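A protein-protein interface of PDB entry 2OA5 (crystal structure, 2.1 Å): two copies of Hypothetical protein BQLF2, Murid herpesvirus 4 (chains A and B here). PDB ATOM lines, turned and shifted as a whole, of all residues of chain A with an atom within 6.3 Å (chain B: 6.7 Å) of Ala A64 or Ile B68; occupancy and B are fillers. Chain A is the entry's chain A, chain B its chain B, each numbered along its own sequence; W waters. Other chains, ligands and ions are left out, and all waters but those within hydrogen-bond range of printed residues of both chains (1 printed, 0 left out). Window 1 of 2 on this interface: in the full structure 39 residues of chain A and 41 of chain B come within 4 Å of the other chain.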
ATOM      1  N   SER A  56       8.637  29.860 -15.027  1.00  0.00           N
ATOM      2  CA  SER A  56       8.219  28.523 -15.445  1.00  0.00           C
ATOM      3  C   SER A  56       6.815  28.592 -16.032  1.00  0.00           C
ATOM      4  O   SER A  56       6.523  27.988 -17.066  1.00  0.00           O
ATOM      5  CB  SER A  56       8.244  27.555 -14.261  1.00  0.00           C
ATOM      6  OG  SER A  56       9.568  27.351 -13.798  1.00  0.00           O
ATOM      7  N   SER A  57       5.946  29.350 -15.371  1.00  0.00           N
ATOM      8  CA  SER A  57       4.578  29.491 -15.829  1.00  0.00           C
ATOM      9  C   SER A  57       4.542  30.154 -17.196  1.00  0.00           C
ATOM     10  O   SER A  57       3.748  29.774 -18.061  1.00  0.00           O
ATOM     11  CB  SER A  57       3.767  30.301 -14.821  1.00  0.00           C
ATOM     12  OG  SER A  57       3.702  29.610 -13.587  1.00  0.00           O
ATOM     13  N   ARG A  58       5.408  31.140 -17.404  1.00  0.00           N
ATOM     14  CA  ARG A  58       5.435  31.819 -18.683  1.00  0.00           C
ATOM     15  C   ARG A  58       5.875  30.901 -19.807  1.00  0.00           C
ATOM     16  O   ARG A  58       5.306  30.941 -20.897  1.00  0.00           O
ATOM     17  CB  ARG A  58       6.283  33.095 -18.605  1.00  0.00           C
ATOM     18  CG  ARG A  58       5.605  34.134 -17.723  1.00  0.00           C
ATOM     19  CD  ARG A  58       6.283  35.500 -17.737  1.00  0.00           C
ATOM     20  NE  ARG A  58       5.489  36.494 -17.015  1.00  0.00           N
ATOM     21  CZ  ARG A  58       5.973  37.648 -16.551  1.00  0.00           C
ATOM     22  NH1 ARG A  58       7.255  37.963 -16.726  1.00  0.00           N
ATOM     23  NH2 ARG A  58       5.169  38.487 -15.915  1.00  0.00           N
ATOM     24  N   ALA A  59       6.857  30.050 -19.525  1.00  0.00           N
ATOM     25  CA  ALA A  59       7.337  29.083 -20.503  1.00  0.00           C
ATOM     26  C   ALA A  59       6.182  28.120 -20.849  1.00  0.00           C
ATOM     27  O   ALA A  59       5.910  27.871 -22.028  1.00  0.00           O
ATOM     28  CB  ALA A  59       8.517  28.306 -19.934  1.00  0.00           C
ATOM     29  N   LEU A  60       5.525  27.573 -19.822  1.00  0.00           N
ATOM     30  CA  LEU A  60       4.379  26.674 -20.023  1.00  0.00           C
ATOM     31  C   LEU A  60       3.298  27.427 -20.785  1.00  0.00           C
ATOM     32  O   LEU A  60       2.722  26.903 -21.732  1.00  0.00           O
ATOM     33  CB  LEU A  60       3.815  26.188 -18.686  1.00  0.00           C
ATOM     34  CG  LEU A  60       4.733  25.203 -17.958  1.00  0.00           C
ATOM     35  CD1 LEU A  60       4.208  24.897 -16.564  1.00  0.00           C
ATOM     36  CD2 LEU A  60       4.890  23.921 -18.787  1.00  0.00           C
ATOM     37  N   GLY A  61       3.024  28.658 -20.373  1.00  0.00           N
ATOM     38  CA  GLY A  61       2.024  29.468 -21.051  1.00  0.00           C
ATOM     39  C   GLY A  61       2.350  29.656 -22.526  1.00  0.00           C
ATOM     40  O   GLY A  61       1.451  29.815 -23.364  1.00  0.00           O
ATOM     41  N   ALA A  62       3.639  29.647 -22.853  1.00  0.00           N
ATOM     42  CA  ALA A  62       4.067  29.800 -24.243  1.00  0.00           C
ATOM     43  C   ALA A  62       3.713  28.537 -25.036  1.00  0.00           C
ATOM     44  O   ALA A  62       3.275  28.611 -26.181  1.00  0.00           O
ATOM     45  CB  ALA A  62       5.574  30.059 -24.306  1.00  0.00           C
ATOM     46  N   VAL A  63       3.923  27.377 -24.425  1.00  0.00           N
ATOM     47  CA  VAL A  63       3.594  26.110 -25.062  1.00  0.00           C
ATOM     48  C   VAL A  63       2.066  26.072 -25.282  1.00  0.00           C
ATOM     49  O   VAL A  63       1.592  25.693 -26.350  1.00  0.00           O
ATOM     50  CB  VAL A  63       4.017  24.920 -24.171  1.00  0.00           C
ATOM     51  CG1 VAL A  63       3.720  23.615 -24.873  1.00  0.00           C
ATOM     52  CG2 VAL A  63       5.509  24.999 -23.851  1.00  0.00           C
ATOM     53  N   ALA A  64       1.307  26.476 -24.266  1.00  0.00           N
ATOM     54  CA  ALA A  64      -0.147  26.509 -24.360  1.00  0.00           C
ATOM     55  C   ALA A  64      -0.576  27.457 -25.487  1.00  0.00           C
ATOM     56  O   ALA A  64      -1.468  27.140 -26.276  1.00  0.00           O
ATOM     57  CB  ALA A  64      -0.753  26.973 -23.029  1.00  0.00           C
ATOM     58  N   MET A  65       0.062  28.619 -25.565  1.00  0.00           N
ATOM     59  CA  MET A  65      -0.267  29.600 -26.598  1.00  0.00           C
ATOM     60  C   MET A  65      -0.179  29.024 -28.008  1.00  0.00           C
ATOM     61  O   MET A  65      -1.125  29.153 -28.797  1.00  0.00           O
ATOM     62  CB  MET A  65       0.659  30.811 -26.501  1.00  0.00           C
ATOM     63  CG  MET A  65       0.298  31.975 -27.442  1.00  0.00           C
ATOM     64  SD  MET A  65      -1.574  32.576 -27.445  1.00  0.00           S
ATOM     65  CE  MET A  65      -1.640  33.658 -25.806  1.00  0.00           C
ATOM     66  N   ARG A  66       0.949  28.391 -28.336  1.00  0.00           N
ATOM     67  CA  ARG A  66       1.101  27.815 -29.667  1.00  0.00           C
ATOM     68  C   ARG A  66       0.178  26.619 -29.909  1.00  0.00           C
ATOM     69  O   ARG A  66      -0.288  26.412 -31.036  1.00  0.00           O
ATOM     70  CB  ARG A  66       2.574  27.455 -29.980  1.00  0.00           C
ATOM     71  CG  ARG A  66       3.334  26.532 -29.021  1.00  0.00           C
ATOM     72  CD  ARG A  66       4.842  26.506 -29.418  1.00  0.00           C
ATOM     73  NE  ARG A  66       5.740  25.767 -28.521  1.00  0.00           N
ATOM     74  CZ  ARG A  66       5.763  24.438 -28.394  1.00  0.00           C
ATOM     75  NH1 ARG A  66       4.935  23.677 -29.108  1.00  0.00           N
ATOM     76  NH2 ARG A  66       6.626  23.864 -27.565  1.00  0.00           N
ATOM     77  N   LYS A  67      -0.090  25.824 -28.872  1.00  0.00           N
ATOM     78  CA  LYS A  67      -1.014  24.698 -29.047  1.00  0.00           C
ATOM     79  C   LYS A  67      -2.435  25.242 -29.277  1.00  0.00           C
ATOM     80  O   LYS A  67      -3.159  24.764 -30.152  1.00  0.00           O
ATOM     81  CB  LYS A  67      -1.009  23.754 -27.836  1.00  0.00           C
ATOM     82  CG  LYS A  67       0.216  22.870 -27.742  1.00  0.00           C
ATOM     83  CD  LYS A  67       0.035  21.779 -26.698  1.00  0.00           C
ATOM     84  CE  LYS A  67       1.276  20.881 -26.623  1.00  0.00           C
ATOM     85  NZ  LYS A  67       1.112  19.729 -25.685  1.00  0.00           N
ATOM     86  N   ILE A  68      -2.820  26.256 -28.509  1.00  0.00           N
ATOM     87  CA  ILE A  68      -4.144  26.852 -28.650  1.00  0.00           C
ATOM     88  C   ILE A  68      -4.370  27.474 -30.032  1.00  0.00           C
ATOM     89  O   ILE A  68      -5.412  27.259 -30.660  1.00  0.00           O
ATOM     90  CB  ILE A  68      -4.390  27.907 -27.567  1.00  0.00           C
ATOM     91  CG1 ILE A  68      -4.681  27.204 -26.226  1.00  0.00           C
ATOM     92  CG2 ILE A  68      -5.513  28.836 -27.997  1.00  0.00           C
ATOM     93  CD1 ILE A  68      -4.667  28.100 -25.005  1.00  0.00           C
ATOM     94  N   GLU A  69      -3.405  28.247 -30.512  1.00  0.00           N
ATOM     95  CA  GLU A  69      -3.570  28.850 -31.827  1.00  0.00           C
ATOM     96  C   GLU A  69      -3.706  27.767 -32.898  1.00  0.00           C
ATOM     97  O   GLU A  69      -4.500  27.902 -33.819  1.00  0.00           O
ATOM     98  CB  GLU A  69      -2.396  29.767 -32.178  1.00  0.00           C
ATOM     99  CG  GLU A  69      -2.532  30.384 -33.568  1.00  0.00           C
ATOM    100  CD  GLU A  69      -1.618  31.573 -33.802  1.00  0.00           C
ATOM    101  OE1 GLU A  69      -1.124  32.162 -32.820  1.00  0.00           O
ATOM    102  OE2 GLU A  69      -1.406  31.936 -34.976  1.00  0.00           O
ATOM    103  N   VAL A  96      -6.019  21.674 -23.303  1.00  0.00           N
ATOM    104  CA  VAL A  96      -4.624  21.793 -23.690  1.00  0.00           C
ATOM    105  C   VAL A  96      -3.724  21.138 -22.669  1.00  0.00           C
ATOM    106  O   VAL A  96      -3.875  21.359 -21.477  1.00  0.00           O
ATOM    107  CB  VAL A  96      -4.219  23.279 -23.822  1.00  0.00           C
ATOM    108  CG1 VAL A  96      -2.813  23.390 -24.349  1.00  0.00           C
ATOM    109  CG2 VAL A  96      -5.180  24.002 -24.744  1.00  0.00           C
ATOM    110  N   ASP A  97      -2.788  20.325 -23.149  1.00  0.00           N
ATOM    111  CA  ASP A  97      -1.823  19.670 -22.282  1.00  0.00           C
ATOM    112  C   ASP A  97      -0.482  20.347 -22.490  1.00  0.00           C
ATOM    113  O   ASP A  97      -0.058  20.530 -23.621  1.00  0.00           O
ATOM    114  CB  ASP A  97      -1.669  18.184 -22.636  1.00  0.00           C
ATOM    115  CG  ASP A  97      -2.902  17.382 -22.319  1.00  0.00           C
ATOM    116  OD1 ASP A  97      -3.411  17.506 -21.183  1.00  0.00           O
ATOM    117  OD2 ASP A  97      -3.356  16.627 -23.202  1.00  0.00           O
ATOM    118  N   VAL A  98       0.169  20.737 -21.393  1.00  0.00           N
ATOM    119  CA  VAL A  98       1.492  21.356 -21.465  1.00  0.00           C
ATOM    120  C   VAL A  98       2.355  20.713 -20.393  1.00  0.00           C
ATOM    121  O   VAL A  98       1.890  20.432 -19.286  1.00  0.00           O
ATOM    122  CB  VAL A  98       1.455  22.888 -21.227  1.00  0.00           C
ATOM    123  CG1 VAL A  98       0.619  23.558 -22.279  1.00  0.00           C
ATOM    124  CG2 VAL A  98       0.901  23.191 -19.867  1.00  0.00           C
ATOM    125  N   GLY B  61      -5.296  32.162 -24.904  1.00  0.00           N
ATOM    126  CA  GLY B  61      -3.964  31.970 -24.347  1.00  0.00           C
ATOM    127  C   GLY B  61      -3.853  32.604 -22.974  1.00  0.00           C
ATOM    128  O   GLY B  61      -3.341  31.998 -22.029  1.00  0.00           O
ATOM    129  N   VAL B  63      -6.162  33.129 -20.858  1.00  0.00           N
ATOM    130  CA  VAL B  63      -6.935  32.367 -19.879  1.00  0.00           C
ATOM    131  C   VAL B  63      -6.115  31.157 -19.448  1.00  0.00           C
ATOM    132  O   VAL B  63      -6.007  30.849 -18.260  1.00  0.00           O
ATOM    133  CB  VAL B  63      -8.281  31.885 -20.478  1.00  0.00           C
ATOM    134  CG1 VAL B  63      -8.870  30.772 -19.617  1.00  0.00           C
ATOM    135  CG2 VAL B  63      -9.256  33.038 -20.552  1.00  0.00           C
ATOM    136  N   ALA B  64      -5.542  30.461 -20.426  1.00  0.00           N
ATOM    137  CA  ALA B  64      -4.724  29.292 -20.131  1.00  0.00           C
ATOM    138  C   ALA B  64      -3.541  29.714 -19.250  1.00  0.00           C
ATOM    139  O   ALA B  64      -3.157  29.018 -18.316  1.00  0.00           O
ATOM    140  CB  ALA B  64      -4.214  28.671 -21.426  1.00  0.00           C
ATOM    141  N   MET B  65      -2.981  30.877 -19.548  1.00  0.00           N
ATOM    142  CA  MET B  65      -1.837  31.371 -18.799  1.00  0.00           C
ATOM    143  C   MET B  65      -2.169  31.604 -17.317  1.00  0.00           C
ATOM    144  O   MET B  65      -1.361  31.287 -16.433  1.00  0.00           O
ATOM    145  CB  MET B  65      -1.311  32.643 -19.470  1.00  0.00           C
ATOM    146  CG  MET B  65       0.123  32.511 -19.967  1.00  0.00           C
ATOM    147  SD  MET B  65       1.319  32.240 -18.494  1.00  0.00           S
ATOM    148  CE  MET B  65       2.919  32.842 -19.322  1.00  0.00           C
ATOM    149  N   ARG B  66      -3.363  32.136 -17.059  1.00  0.00           N
ATOM    150  CA  ARG B  66      -3.844  32.399 -15.703  1.00  0.00           C
ATOM    151  C   ARG B  66      -3.911  31.078 -14.938  1.00  0.00           C
ATOM    152  O   ARG B  66      -3.345  30.932 -13.855  1.00  0.00           O
ATOM    153  CB  ARG B  66      -5.242  33.031 -15.766  1.00  0.00           C
ATOM    154  CG  ARG B  66      -6.092  32.884 -14.498  1.00  0.00           C
ATOM    155  CD  ARG B  66      -7.578  32.797 -14.854  1.00  0.00           C
ATOM    156  NE  ARG B  66      -8.005  33.923 -15.682  1.00  0.00           N
ATOM    157  CZ  ARG B  66      -9.193  34.019 -16.271  1.00  0.00           C
ATOM    158  NH1 ARG B  66     -10.092  33.053 -16.129  1.00  0.00           N
ATOM    159  NH2 ARG B  66      -9.486  35.084 -17.007  1.00  0.00           N
ATOM    160  N   LYS B  67      -4.607  30.118 -15.538  1.00  0.00           N
ATOM    161  CA  LYS B  67      -4.804  28.797 -14.959  1.00  0.00           C
ATOM    162  C   LYS B  67      -3.510  28.021 -14.740  1.00  0.00           C
ATOM    163  O   LYS B  67      -3.342  27.348 -13.724  1.00  0.00           O
ATOM    164  CB  LYS B  67      -5.750  27.981 -15.854  1.00  0.00           C
ATOM    165  CG  LYS B  67      -7.107  28.632 -16.090  1.00  0.00           C
ATOM    166  CD  LYS B  67      -8.083  27.662 -16.750  1.00  0.00           C
ATOM    167  CE  LYS B  67      -9.488  28.249 -16.795  1.00  0.00           C
ATOM    168  NZ  LYS B  67     -10.522  27.227 -16.465  1.00  0.00           N
ATOM    169  N   ILE B  68      -2.599  28.104 -15.704  1.00  0.00           N
ATOM    170  CA  ILE B  68      -1.325  27.407 -15.605  1.00  0.00           C
ATOM    171  C   ILE B  68      -0.508  27.894 -14.405  1.00  0.00           C
ATOM    172  O   ILE B  68       0.027  27.097 -13.640  1.00  0.00           O
ATOM    173  CB  ILE B  68      -0.509  27.591 -16.905  1.00  0.00           C
ATOM    174  CG1 ILE B  68      -1.062  26.650 -17.981  1.00  0.00           C
ATOM    175  CG2 ILE B  68       0.966  27.331 -16.649  1.00  0.00           C
ATOM    176  CD1 ILE B  68      -0.753  27.074 -19.399  1.00  0.00           C
ATOM    177  N   GLU B  69      -0.419  29.207 -14.254  1.00  0.00           N
ATOM    178  CA  GLU B  69       0.324  29.792 -13.152  1.00  0.00           C
ATOM    179  C   GLU B  69      -0.215  29.287 -11.817  1.00  0.00           C
ATOM    180  O   GLU B  69       0.544  28.950 -10.904  1.00  0.00           O
ATOM    181  CB  GLU B  69       0.189  31.308 -13.202  1.00  0.00           C
ATOM    182  CG  GLU B  69       1.160  32.048 -12.314  1.00  0.00           C
ATOM    183  CD  GLU B  69       0.906  33.534 -12.329  1.00  0.00           C
ATOM    184  OE1 GLU B  69       0.563  34.067 -13.407  1.00  0.00           O
ATOM    185  OE2 GLU B  69       1.052  34.174 -11.271  1.00  0.00           O
ATOM    186  N   ALA B  70      -1.543  29.255 -11.717  1.00  0.00           N
ATOM    187  CA  ALA B  70      -2.223  28.808 -10.511  1.00  0.00           C
ATOM    188  C   ALA B  70      -1.790  27.402 -10.106  1.00  0.00           C
ATOM    189  O   ALA B  70      -1.490  27.145  -8.941  1.00  0.00           O
ATOM    190  CB  ALA B  70      -3.736  28.854 -10.732  1.00  0.00           C
ATOM    191  N   LYS B  71      -1.755  26.497 -11.077  1.00  0.00           N
ATOM    192  CA  LYS B  71      -1.370  25.112 -10.835  1.00  0.00           C
ATOM    193  C   LYS B  71       0.112  24.979 -10.529  1.00  0.00           C
ATOM    194  O   LYS B  71       0.525  24.114  -9.754  1.00  0.00           O
ATOM    195  CB  LYS B  71      -1.750  24.257 -12.047  1.00  0.00           C
ATOM    196  CG  LYS B  71      -3.220  24.384 -12.391  1.00  0.00           C
ATOM    197  CD  LYS B  71      -3.656  23.440 -13.484  1.00  0.00           C
ATOM    198  CE  LYS B  71      -4.773  22.551 -12.966  1.00  0.00           C
ATOM    199  NZ  LYS B  71      -5.637  22.024 -14.057  1.00  0.00           N
ATOM    200  N   VAL B  72       0.924  25.837 -11.146  1.00  0.00           N
ATOM    201  CA  VAL B  72       2.355  25.808 -10.892  1.00  0.00           C
ATOM    202  C   VAL B  72       2.540  26.292  -9.455  1.00  0.00           C
ATOM    203  O   VAL B  72       3.298  25.705  -8.691  1.00  0.00           O
ATOM    204  CB  VAL B  72       3.129  26.726 -11.885  1.00  0.00           C
ATOM    205  CG1 VAL B  72       4.614  26.793 -11.503  1.00  0.00           C
ATOM    206  CG2 VAL B  72       2.973  26.185 -13.309  1.00  0.00           C
ATOM    207  N   ARG B  73       1.826  27.351  -9.080  1.00  0.00           N
ATOM    208  CA  ARG B  73       1.926  27.858  -7.715  1.00  0.00           C
ATOM    209  C   ARG B  73       1.578  26.763  -6.718  1.00  0.00           C
ATOM    210  O   ARG B  73       2.275  26.559  -5.726  1.00  0.00           O
ATOM    211  CB  ARG B  73       0.994  29.048  -7.504  1.00  0.00           C
ATOM    212  CG  ARG B  73       1.616  30.370  -7.856  1.00  0.00           C
ATOM    213  CD  ARG B  73       0.709  31.532  -7.501  1.00  0.00           C
ATOM    214  NE  ARG B  73       1.479  32.771  -7.483  1.00  0.00           N
ATOM    215  CZ  ARG B  73       2.193  33.211  -8.513  1.00  0.00           C
ATOM    216  NH1 ARG B  73       2.224  32.518  -9.641  1.00  0.00           N
ATOM    217  NH2 ARG B  73       2.898  34.326  -8.415  1.00  0.00           N
ATOM    218  N   LEU B  92       6.614  17.906 -14.406  1.00  0.00           N
ATOM    219  CA  LEU B  92       5.299  18.528 -14.390  1.00  0.00           C
ATOM    220  C   LEU B  92       4.537  18.469 -15.712  1.00  0.00           C
ATOM    221  O   LEU B  92       5.080  18.758 -16.786  1.00  0.00           O
ATOM    222  CB  LEU B  92       5.410  19.994 -13.943  1.00  0.00           C
ATOM    223  CG  LEU B  92       4.061  20.717 -13.870  1.00  0.00           C
ATOM    224  CD1 LEU B  92       3.306  20.166 -12.671  1.00  0.00           C
ATOM    225  CD2 LEU B  92       4.229  22.216 -13.729  1.00  0.00           C
ATOM    226  N   LEU B  94       0.508  19.538 -16.943  1.00  0.00           N
ATOM    227  CA  LEU B  94      -0.753  20.120 -16.528  1.00  0.00           C
ATOM    228  C   LEU B  94      -1.753  19.989 -17.638  1.00  0.00           C
ATOM    229  O   LEU B  94      -1.391  19.872 -18.807  1.00  0.00           O
ATOM    230  CB  LEU B  94      -0.606  21.616 -16.258  1.00  0.00           C
ATOM    231  CG  LEU B  94       0.460  22.216 -15.349  1.00  0.00           C
ATOM    232  CD1 LEU B  94       0.250  23.724 -15.306  1.00  0.00           C
ATOM    233  CD2 LEU B  94       0.368  21.629 -13.951  1.00  0.00           C
ATOM    234  N   ARG B  95      -3.027  19.987 -17.279  1.00  0.00           N
ATOM    235  CA  ARG B  95      -4.027  19.982 -18.315  1.00  0.00           C
ATOM    236  C   ARG B  95      -4.864  21.206 -18.031  1.00  0.00           C
ATOM    237  O   ARG B  95      -5.197  21.499 -16.883  1.00  0.00           O
ATOM    238  CB  ARG B  95      -4.887  18.733 -18.321  1.00  0.00           C
ATOM    239  CG  ARG B  95      -5.646  18.656 -19.636  1.00  0.00           C
ATOM    240  CD  ARG B  95      -6.722  17.604 -19.631  1.00  0.00           C
ATOM    241  NE  ARG B  95      -6.236  16.272 -19.964  1.00  0.00           N
ATOM    242  CZ  ARG B  95      -5.806  15.903 -21.169  1.00  0.00           C
ATOM    243  NH1 ARG B  95      -5.792  16.772 -22.171  1.00  0.00           N
ATOM    244  NH2 ARG B  95      -5.405  14.657 -21.371  1.00  0.00           N
ATOM    245  N   VAL B  96      -5.172  21.938 -19.093  1.00  0.00           N
ATOM    246  CA  VAL B  96      -5.928  23.173 -18.981  1.00  0.00           C
ATOM    247  C   VAL B  96      -7.070  23.263 -19.981  1.00  0.00           C
ATOM    248  O   VAL B  96      -6.921  22.939 -21.160  1.00  0.00           O
ATOM    249  CB  VAL B  96      -4.969  24.377 -19.168  1.00  0.00           C
ATOM    250  CG1 VAL B  96      -5.735  25.627 -19.541  1.00  0.00           C
ATOM    251  CG2 VAL B  96      -4.190  24.607 -17.886  1.00  0.00           C
HETATM  252  O   HOH W   1      -1.013  30.535 -22.903  1.00  0.00           O
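N of Val A96 lies within hydrogen-bond range of O of Val B96.
The side-chain carboxylate (OD2) of Asp A97 lies within salt-bridge range of the guanidinium group (NH1) of Arg B95 (2.6 Å).
The backbone carbonyl oxygen of Val A98 sits at hydrogen-bond distance from the backbone NH of Leu B94, at 2.9 Å.
The side-chain sulfur (SD) of Met B65 sits close to the backbone carbonyl oxygen (O) of Ser A57 (3.5 Å).
NZ of Lys A67 is in hydrogen-bond range of O of Asp A97 (2.5 Å).
OE2 of Glu B69 lies within salt-bridge range of NH1 of Arg B73 (2.6 Å).
The side-chain amino group of Lys B71 sits at hydrogen-bond distance from the backbone carbonyl oxygen of Arg B95 (2.9 Å).
Among the printed residues, pairs that only touch across the chains: Ser A57 with Ile B68 (3.96 Å), Ser A57 with Glu B69 (3.4 Å), Ser A57 with Val B72 (3.4 Å), Arg A58 with Met B65 (2.8 Å), Leu A60 with Ile B68 (3.7 Å), Leu A60 with Val B72 (3.7 Å), Leu A60 with Leu B92 (3.9 Å), Gly A61 with Met B65 (3.7 Å), Ala A64 with Ile B68 (3.6 Å), Met A65 with Gly B61 (3.2 Å), Ile A68 with Gly B61 (3.99 Å), Ile A68 with Ala B64 (3.7 Å), Val A96 with Leu B94 (3.9 Å), Val A96 with Arg B95 (3.5 Å) and Asp A97 with Leu B94 (3.5 Å).
Printed residues of chain B within 4 Å of Ala A64: Ile B68 (3.6 Å).
Printed residues of chain B within 4 Å of Met A65: Gly B61.
Printed residues of chain A within 4 Å of Leu B94: Val A96 (3.9 Å), Asp A97 (3.5 Å) and Val A98 (2.9 Å).
Of the printed residues of chain A, Arg B95 touches Val A96 (3.5 Å) and Asp A97 (2.6 Å).
Of the printed residues of chain A, Val B96 touches Val A96 (2.6 Å).
The nearest residue of chain B that does not touch Ala A64 is Ala B64 (4.2 Å).
The nearest printed residue of chain A that does not touch Val B96 is Asp A97 (5.0 Å).
Of the 16 printed residues of chain B, 10 touch a printed residue of chain A.
Hydrophobic or aromatic side chains of chain B within 4 Å of the printed part of chain A: Ala B64, Met B65, Ile B68, Val B72, Leu B92 and Val B96.
Of the 17 printed residues of chain A, 10 touch a printed residue of chain B.
Gly A61 touches Met B65, and with the chains exchanged Met A65 touches Gly B61.
Ala A64 touches Ile B68, and with the chains exchanged Ile A68 touches Ala B64.
Ile A68 touches Gly B61, but with the chains exchanged Gly A61 does not touch Ile B68 (4.02 Å).
Val B96 touches its own counterpart, Val A96.
9 positions are printed for both chains.
Of the 19 pairs that touch across the chains among the printed residues, 5 have their exchanged pair printed and touching as well.
Water W1 lies within hydrogen-bond range of the backbone carbonyl oxygen (O) of Gly A61 (2.6 Å), the backbone carbonyl oxygen (O) of Gly B61 (2.9 Å) and the backbone NH (N) of Met A65 (3.5 Å).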
